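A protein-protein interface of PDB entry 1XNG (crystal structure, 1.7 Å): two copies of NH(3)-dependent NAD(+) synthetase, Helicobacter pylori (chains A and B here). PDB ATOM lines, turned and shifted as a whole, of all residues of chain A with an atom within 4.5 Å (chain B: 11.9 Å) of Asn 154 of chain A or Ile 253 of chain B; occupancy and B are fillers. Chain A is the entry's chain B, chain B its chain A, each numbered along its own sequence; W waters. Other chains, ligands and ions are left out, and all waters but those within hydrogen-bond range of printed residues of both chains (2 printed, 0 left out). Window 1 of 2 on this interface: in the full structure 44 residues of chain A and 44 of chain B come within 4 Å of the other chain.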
ATOM      1  N   PHE A  15      37.785  17.067 -18.901  1.00  0.00           N
ATOM      2  CA  PHE A  15      36.624  16.189 -18.815  1.00  0.00           C
ATOM      3  C   PHE A  15      37.065  14.742 -18.990  1.00  0.00           C
ATOM      4  O   PHE A  15      36.701  13.870 -18.202  1.00  0.00           O
ATOM      5  CB  PHE A  15      35.617  16.543 -19.914  1.00  0.00           C
ATOM      6  CG  PHE A  15      34.514  15.534 -20.080  1.00  0.00           C
ATOM      7  CD1 PHE A  15      33.431  15.516 -19.206  1.00  0.00           C
ATOM      8  CD2 PHE A  15      34.567  14.592 -21.104  1.00  0.00           C
ATOM      9  CE1 PHE A  15      32.414  14.573 -19.346  1.00  0.00           C
ATOM     10  CE2 PHE A  15      33.558  13.642 -21.256  1.00  0.00           C
ATOM     11  CZ  PHE A  15      32.477  13.634 -20.373  1.00  0.00           C
ATOM     12  N   GLY A 131      33.472   7.585 -26.952  1.00  0.00           N
ATOM     13  CA  GLY A 131      32.573   7.794 -28.073  1.00  0.00           C
ATOM     14  C   GLY A 131      32.916   9.005 -28.914  1.00  0.00           C
ATOM     15  O   GLY A 131      33.692   9.861 -28.498  1.00  0.00           O
ATOM     16  N   THR A 132      32.310   9.092 -30.096  1.00  0.00           N
ATOM     17  CA  THR A 132      32.590  10.186 -31.016  1.00  0.00           C
ATOM     18  C   THR A 132      31.355  10.790 -31.679  1.00  0.00           C
ATOM     19  O   THR A 132      31.482  11.518 -32.664  1.00  0.00           O
ATOM     20  CB  THR A 132      33.496   9.709 -32.149  1.00  0.00           C
ATOM     21  OG1 THR A 132      32.756   8.811 -32.986  1.00  0.00           O
ATOM     22  CG2 THR A 132      34.709   8.982 -31.590  1.00  0.00           C
ATOM     23  N   SER A 133      30.172  10.480 -31.164  1.00  0.00           N
ATOM     24  CA  SER A 133      28.939  11.010 -31.739  1.00  0.00           C
ATOM     25  C   SER A 133      28.776  12.479 -31.355  1.00  0.00           C
ATOM     26  O   SER A 133      28.791  12.813 -30.172  1.00  0.00           O
ATOM     27  CB  SER A 133      27.737  10.207 -31.235  1.00  0.00           C
ATOM     28  OG  SER A 133      27.845   8.843 -31.604  1.00  0.00           O
ATOM     29  N   ARG A 138      23.489  13.140 -32.529  1.00  0.00           N
ATOM     30  CA  ARG A 138      22.686  12.705 -31.389  1.00  0.00           C
ATOM     31  C   ARG A 138      21.239  13.206 -31.455  1.00  0.00           C
ATOM     32  O   ARG A 138      20.303  12.424 -31.313  1.00  0.00           O
ATOM     33  CB  ARG A 138      23.360  13.120 -30.072  1.00  0.00           C
ATOM     34  CG  ARG A 138      24.614  12.289 -29.773  1.00  0.00           C
ATOM     35  CD  ARG A 138      25.378  12.775 -28.543  1.00  0.00           C
ATOM     36  NE  ARG A 138      24.606  12.651 -27.309  1.00  0.00           N
ATOM     37  CZ  ARG A 138      24.286  11.500 -26.724  1.00  0.00           C
ATOM     38  NH1 ARG A 138      24.668  10.342 -27.252  1.00  0.00           N
ATOM     39  NH2 ARG A 138      23.582  11.509 -25.601  1.00  0.00           N
ATOM     40  N   CYS A 151      29.270   3.740 -25.893  1.00  0.00           N
ATOM     41  CA  CYS A 151      30.554   4.125 -25.304  1.00  0.00           C
ATOM     42  C   CYS A 151      30.432   4.379 -23.804  1.00  0.00           C
ATOM     43  O   CYS A 151      29.337   4.343 -23.240  1.00  0.00           O
ATOM     44  CB  CYS A 151      31.095   5.398 -25.970  1.00  0.00           C
ATOM     45  SG  CYS A 151      30.211   6.927 -25.509  1.00  0.00           S
ATOM     46  N   ILE A 153      32.281   7.218 -22.239  1.00  0.00           N
ATOM     47  CA  ILE A 153      32.297   8.679 -22.152  1.00  0.00           C
ATOM     48  C   ILE A 153      32.463   9.241 -23.554  1.00  0.00           C
ATOM     49  O   ILE A 153      33.155   8.657 -24.389  1.00  0.00           O
ATOM     50  CB  ILE A 153      33.466   9.215 -21.272  1.00  0.00           C
ATOM     51  CG1 ILE A 153      34.814   8.862 -21.905  1.00  0.00           C
ATOM     52  CG2 ILE A 153      33.373   8.641 -19.861  1.00  0.00           C
ATOM     53  CD1 ILE A 153      36.010   9.537 -21.226  1.00  0.00           C
ATOM     54  N   ASN A 154      31.820  10.376 -23.803  1.00  0.00           N
ATOM     55  CA  ASN A 154      31.872  11.031 -25.104  1.00  0.00           C
ATOM     56  C   ASN A 154      32.118  12.520 -24.890  1.00  0.00           C
ATOM     57  O   ASN A 154      31.244  13.241 -24.418  1.00  0.00           O
ATOM     58  CB  ASN A 154      30.545  10.813 -25.827  1.00  0.00           C
ATOM     59  CG  ASN A 154      30.472  11.524 -27.160  1.00  0.00           C
ATOM     60  OD1 ASN A 154      31.405  12.212 -27.576  1.00  0.00           O
ATOM     61  ND2 ASN A 154      29.343  11.365 -27.836  1.00  0.00           N
ATOM     62  N   PRO A 155      33.315  13.001 -25.247  1.00  0.00           N
ATOM     63  CA  PRO A 155      33.682  14.407 -25.087  1.00  0.00           C
ATOM     64  C   PRO A 155      33.054  15.398 -26.053  1.00  0.00           C
ATOM     65  O   PRO A 155      33.038  16.592 -25.771  1.00  0.00           O
ATOM     66  CB  PRO A 155      35.198  14.376 -25.222  1.00  0.00           C
ATOM     67  CG  PRO A 155      35.399  13.318 -26.247  1.00  0.00           C
ATOM     68  CD  PRO A 155      34.448  12.228 -25.786  1.00  0.00           C
ATOM     69  N   ILE A 156      32.533  14.926 -27.183  1.00  0.00           N
ATOM     70  CA  ILE A 156      31.958  15.851 -28.154  1.00  0.00           C
ATOM     71  C   ILE A 156      30.451  15.738 -28.365  1.00  0.00           C
ATOM     72  O   ILE A 156      29.907  16.322 -29.304  1.00  0.00           O
ATOM     73  CB  ILE A 156      32.672  15.725 -29.526  1.00  0.00           C
ATOM     74  CG1 ILE A 156      32.585  14.287 -30.042  1.00  0.00           C
ATOM     75  CG2 ILE A 156      34.135  16.155 -29.385  1.00  0.00           C
ATOM     76  CD1 ILE A 156      33.053  14.117 -31.483  1.00  0.00           C
ATOM     77  N   GLY A 157      29.783  15.021 -27.467  1.00  0.00           N
ATOM     78  CA  GLY A 157      28.344  14.835 -27.572  1.00  0.00           C
ATOM     79  C   GLY A 157      27.506  16.100 -27.489  1.00  0.00           C
ATOM     80  O   GLY A 157      26.338  16.093 -27.887  1.00  0.00           O
ATOM     81  N   GLU A 158      28.085  17.178 -26.969  1.00  0.00           N
ATOM     82  CA  GLU A 158      27.368  18.445 -26.853  1.00  0.00           C
ATOM     83  C   GLU A 158      27.890  19.519 -27.804  1.00  0.00           C
ATOM     84  O   GLU A 158      27.638  20.713 -27.618  1.00  0.00           O
ATOM     85  CB  GLU A 158      27.402  18.954 -25.410  1.00  0.00           C
ATOM     86  CG  GLU A 158      26.425  18.244 -24.476  1.00  0.00           C
ATOM     87  CD  GLU A 158      24.976  18.356 -24.933  1.00  0.00           C
ATOM     88  OE1 GLU A 158      24.602  19.420 -25.471  1.00  0.00           O
ATOM     89  OE2 GLU A 158      24.207  17.389 -24.741  1.00  0.00           O
ATOM     90  N   PHE B 146      25.326  -3.649 -23.709  1.00  0.00           N
ATOM     91  CA  PHE B 146      25.061  -3.587 -25.146  1.00  0.00           C
ATOM     92  C   PHE B 146      24.911  -4.978 -25.754  1.00  0.00           C
ATOM     93  O   PHE B 146      24.935  -5.146 -26.974  1.00  0.00           O
ATOM     94  CB  PHE B 146      26.154  -2.790 -25.858  1.00  0.00           C
ATOM     95  CG  PHE B 146      26.348  -1.418 -25.296  1.00  0.00           C
ATOM     96  CD1 PHE B 146      27.619  -0.947 -25.004  1.00  0.00           C
ATOM     97  CD2 PHE B 146      25.253  -0.612 -25.007  1.00  0.00           C
ATOM     98  CE1 PHE B 146      27.799   0.306 -24.428  1.00  0.00           C
ATOM     99  CE2 PHE B 146      25.422   0.637 -24.434  1.00  0.00           C
ATOM    100  CZ  PHE B 146      26.696   1.099 -24.143  1.00  0.00           C
ATOM    101  N   PHE B 246      27.680   1.366 -13.592  1.00  0.00           N
ATOM    102  CA  PHE B 246      27.725   2.077 -14.869  1.00  0.00           C
ATOM    103  C   PHE B 246      26.846   1.475 -15.960  1.00  0.00           C
ATOM    104  O   PHE B 246      26.448   2.174 -16.891  1.00  0.00           O
ATOM    105  CB  PHE B 246      29.166   2.139 -15.380  1.00  0.00           C
ATOM    106  CG  PHE B 246      29.707   0.809 -15.840  1.00  0.00           C
ATOM    107  CD1 PHE B 246      29.542   0.388 -17.160  1.00  0.00           C
ATOM    108  CD2 PHE B 246      30.369  -0.032 -14.948  1.00  0.00           C
ATOM    109  CE1 PHE B 246      30.028  -0.846 -17.583  1.00  0.00           C
ATOM    110  CE2 PHE B 246      30.861  -1.268 -15.361  1.00  0.00           C
ATOM    111  CZ  PHE B 246      30.690  -1.676 -16.679  1.00  0.00           C
ATOM    112  N   GLU B 249      23.489   3.131 -16.303  1.00  0.00           N
ATOM    113  CA  GLU B 249      23.544   4.559 -16.563  1.00  0.00           C
ATOM    114  C   GLU B 249      23.888   4.862 -18.013  1.00  0.00           C
ATOM    115  O   GLU B 249      24.398   4.007 -18.737  1.00  0.00           O
ATOM    116  CB  GLU B 249      24.588   5.199 -15.639  1.00  0.00           C
ATOM    117  CG  GLU B 249      24.320   4.967 -14.151  1.00  0.00           C
ATOM    118  CD  GLU B 249      25.547   5.193 -13.274  1.00  0.00           C
ATOM    119  OE1 GLU B 249      25.407   5.141 -12.033  1.00  0.00           O
ATOM    120  OE2 GLU B 249      26.650   5.415 -13.823  1.00  0.00           O
ATOM    121  N   LEU B 250      23.587   6.086 -18.432  1.00  0.00           N
ATOM    122  CA  LEU B 250      23.894   6.537 -19.782  1.00  0.00           C
ATOM    123  C   LEU B 250      25.365   6.948 -19.801  1.00  0.00           C
ATOM    124  O   LEU B 250      25.945   7.249 -18.757  1.00  0.00           O
ATOM    125  CB  LEU B 250      23.022   7.744 -20.140  1.00  0.00           C
ATOM    126  CG  LEU B 250      21.535   7.467 -20.353  1.00  0.00           C
ATOM    127  CD1 LEU B 250      20.737   8.759 -20.315  1.00  0.00           C
ATOM    128  CD2 LEU B 250      21.359   6.754 -21.674  1.00  0.00           C
ATOM    129  N   PRO B 251      25.995   6.956 -20.986  1.00  0.00           N
ATOM    130  CA  PRO B 251      27.405   7.347 -21.064  1.00  0.00           C
ATOM    131  C   PRO B 251      27.581   8.803 -20.652  1.00  0.00           C
ATOM    132  O   PRO B 251      26.675   9.622 -20.838  1.00  0.00           O
ATOM    133  CB  PRO B 251      27.748   7.109 -22.534  1.00  0.00           C
ATOM    134  CG  PRO B 251      26.437   7.329 -23.227  1.00  0.00           C
ATOM    135  CD  PRO B 251      25.472   6.608 -22.317  1.00  0.00           C
ATOM    136  N   ALA B 252      28.736   9.112 -20.074  1.00  0.00           N
ATOM    137  CA  ALA B 252      29.051  10.465 -19.628  1.00  0.00           C
ATOM    138  C   ALA B 252      29.342  11.348 -20.836  1.00  0.00           C
ATOM    139  O   ALA B 252      30.241  11.048 -21.620  1.00  0.00           O
ATOM    140  CB  ALA B 252      30.261  10.445 -18.700  1.00  0.00           C
ATOM    141  N   ILE B 253      28.584  12.431 -20.975  1.00  0.00           N
ATOM    142  CA  ILE B 253      28.763  13.364 -22.086  1.00  0.00           C
ATOM    143  C   ILE B 253      29.139  14.734 -21.533  1.00  0.00           C
ATOM    144  O   ILE B 253      28.475  15.248 -20.634  1.00  0.00           O
ATOM    145  CB  ILE B 253      27.465  13.541 -22.898  1.00  0.00           C
ATOM    146  CG1 ILE B 253      26.831  12.184 -23.205  1.00  0.00           C
ATOM    147  CG2 ILE B 253      27.767  14.290 -24.185  1.00  0.00           C
ATOM    148  CD1 ILE B 253      27.689  11.267 -24.039  1.00  0.00           C
ATOM    149  N   ALA B 254      30.199  15.325 -22.068  1.00  0.00           N
ATOM    150  CA  ALA B 254      30.637  16.640 -21.615  1.00  0.00           C
ATOM    151  C   ALA B 254      29.528  17.662 -21.851  1.00  0.00           C
ATOM    152  O   ALA B 254      29.003  17.767 -22.958  1.00  0.00           O
ATOM    153  CB  ALA B 254      31.893  17.051 -22.363  1.00  0.00           C
ATOM    154  N   LYS B 255      29.167  18.405 -20.809  1.00  0.00           N
ATOM    155  CA  LYS B 255      28.118  19.414 -20.925  1.00  0.00           C
ATOM    156  C   LYS B 255      28.506  20.478 -21.947  1.00  0.00           C
ATOM    157  O   LYS B 255      29.689  20.737 -22.173  1.00  0.00           O
ATOM    158  CB  LYS B 255      27.854  20.060 -19.563  1.00  0.00           C
ATOM    159  N   ARG B 256      27.504  21.092 -22.568  1.00  0.00           N
ATOM    160  CA  ARG B 256      27.761  22.120 -23.567  1.00  0.00           C
ATOM    161  C   ARG B 256      28.559  23.264 -22.948  1.00  0.00           C
ATOM    162  O   ARG B 256      28.133  23.869 -21.964  1.00  0.00           O
ATOM    163  CB  ARG B 256      26.443  22.647 -24.136  1.00  0.00           C
ATOM    164  CG  ARG B 256      26.599  23.388 -25.457  1.00  0.00           C
ATOM    165  CD  ARG B 256      25.258  23.566 -26.137  1.00  0.00           C
ATOM    166  NE  ARG B 256      25.388  23.955 -27.539  1.00  0.00           N
ATOM    167  CZ  ARG B 256      25.877  25.117 -27.955  1.00  0.00           C
ATOM    168  NH1 ARG B 256      26.287  26.020 -27.074  1.00  0.00           N
ATOM    169  NH2 ARG B 256      25.952  25.378 -29.253  1.00  0.00           N
ATOM    170  N   PHE B 257      29.723  23.544 -23.530  1.00  0.00           N
ATOM    171  CA  PHE B 257      30.606  24.608 -23.056  1.00  0.00           C
ATOM    172  C   PHE B 257      29.922  25.967 -23.133  1.00  0.00           C
ATOM    173  O   PHE B 257      29.706  26.493 -24.224  1.00  0.00           O
ATOM    174  CB  PHE B 257      31.892  24.626 -23.879  1.00  0.00           C
HETATM  175  O   HOH W   1      29.650  22.508 -26.346  1.00  0.00           O
HETATM  176  O   HOH W   2      30.449  17.802 -25.556  1.00  0.00           O
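No position is printed for both chains.
Of the 13 pairs that touch across the chains among the printed residues, none has its exchanged pair printed and touching as well.
The backbone carbonyl oxygen (O) of Ala 252 of chain B is in hydrogen-bond range of the backbone NH (N) of Asn 154 of chain A (2.8 Å).
The backbone NH (N) of Ala 254 of chain B sits at hydrogen-bond distance from the backbone carbonyl oxygen (O) of Asn 154 of chain A, 3.3 Å away.
Hydrophobic or aromatic side chains of chain B that line the printed part of chain A: Pro 251, Ala 252, Ile 253 and Ala 254.
Printed residues of chain A that touch a printed residue of chain B: Phe 15, Cys 151, Ile 153, Asn 154, Pro 155, Gly 157 and Glu 158.
Along chain A the printed residues that touch a printed residue of chain B span positions 15 to 158.
Water W2 lies within hydrogen-bond range of N of Glu 158 of chain A, O of Pro 155 of chain A, O of Ala 254 of chain B and N of Gly 157 of chain A.
Water W1 bridges the backbone carbonyl oxygen (O) of Glu 158 of chain A and the backbone NH (N) of Phe 257 of chain B.
The backbone NH of Gly 131 of chain A sits close to the side-chain sulfur of Cys 151 of chain A, at 3.6 Å.
The backbone NH (N) of Gly 131 of chain A lies within hydrogen-bond range of the backbone carbonyl oxygen (O) of Ile 153 of chain A (2.8 Å).
The side-chain amide oxygen (OD1) of Asn 154 of chain A lies close to the backbone carbonyl oxygen (O) of Gly 131 of chain A (3.4 Å).
The side-chain amide nitrogen (ND2) of Asn 154 of chain A sits at hydrogen-bond distance from the backbone carbonyl oxygen (O) of Ser 133 of chain A.
SG of Cys 151 of chain A sits at hydrogen-bond distance from O of Ile 153 of chain A.
The side-chain amide oxygen (OD1) of Asn 154 of chain A is in hydrogen-bond range of the backbone NH (N) of Gly 157 of chain A (3.2 Å).
Of the printed residues of chain B, Phe 15 of chain A touches Ala 252, Ile 253 and Ala 254.
No residue of chain B comes within 4 Å of Thr 132 of chain A.
No residue of chain B comes within 4 Å of Ser 133 of chain A.
Ile 153 of chain A touches just one residue of chain B: Ala 252.
No residue of chain B comes within 4 Å of Ile 156 of chain A.
Printed residues of chain B within 4 Å of Gly 157 of chain A: Ile 253.
Glu 158 of chain A touches just these residues of chain B: Ala 254 (3.0 Å), Lys 255 (3.9 Å) and Arg 256 (3.6 Å).
Phe 246 of chain B touches none of the printed residues of chain A.
Leu 250 of chain B touches none of the printed residues of chain A.
Of the printed residues of chain A, Pro 251 of chain B touches Cys 151.
Of the printed residues of chain A, Ala 252 of chain B touches Phe 15, Ile 153 and Asn 154.
Of chain A, only Phe 15 (3.7 Å), Asn 154 (3.4 Å) and Gly 157 (3.5 Å) come within 4 Å of Ile 253 of chain B.
Printed residues of chain A within 4 Å of Lys 255 of chain B: Glu 158 (3.9 Å).
Printed residues of chain A within 4 Å of Arg 256 of chain B: Glu 158 (3.6 Å).
The nearest residue of chain A that does not touch Ile 253 of chain B is Glu 158 of chain A (4.02 Å).
The nearest printed residue of chain A that does not touch Lys 255 of chain B is Phe 15 of chain A (5.2 Å).
Phe 15 of chain A touches Ala 252 of chain B (CZ to O, 3.6 Å).
Phe 15 of chain A touches Ile 253 of chain B (CZ to C, 3.7 Å).
Phe 15 of chain A touches Ala 254 of chain B (CZ to N, 3.3 Å).
Cys 151 of chain A touches Pro 251 of chain B.
Ile 153 of chain A touches Ala 252 of chain B.
CB of Asn 154 of chain A touches CD1 of Ile 253 of chain B, 3.4 Å away.
Pro 155 of chain A touches Ala 254 of chain B (O to CB, 3.6 Å).
Ile 253 of chain B touches Gly 157 of chain A (CG2 to CA, 3.5 Å).
Glu 158 of chain A touches Ala 254 of chain B.
Arg 256 of chain B touches Glu 158 of chain A (N to CB, 3.6 Å).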
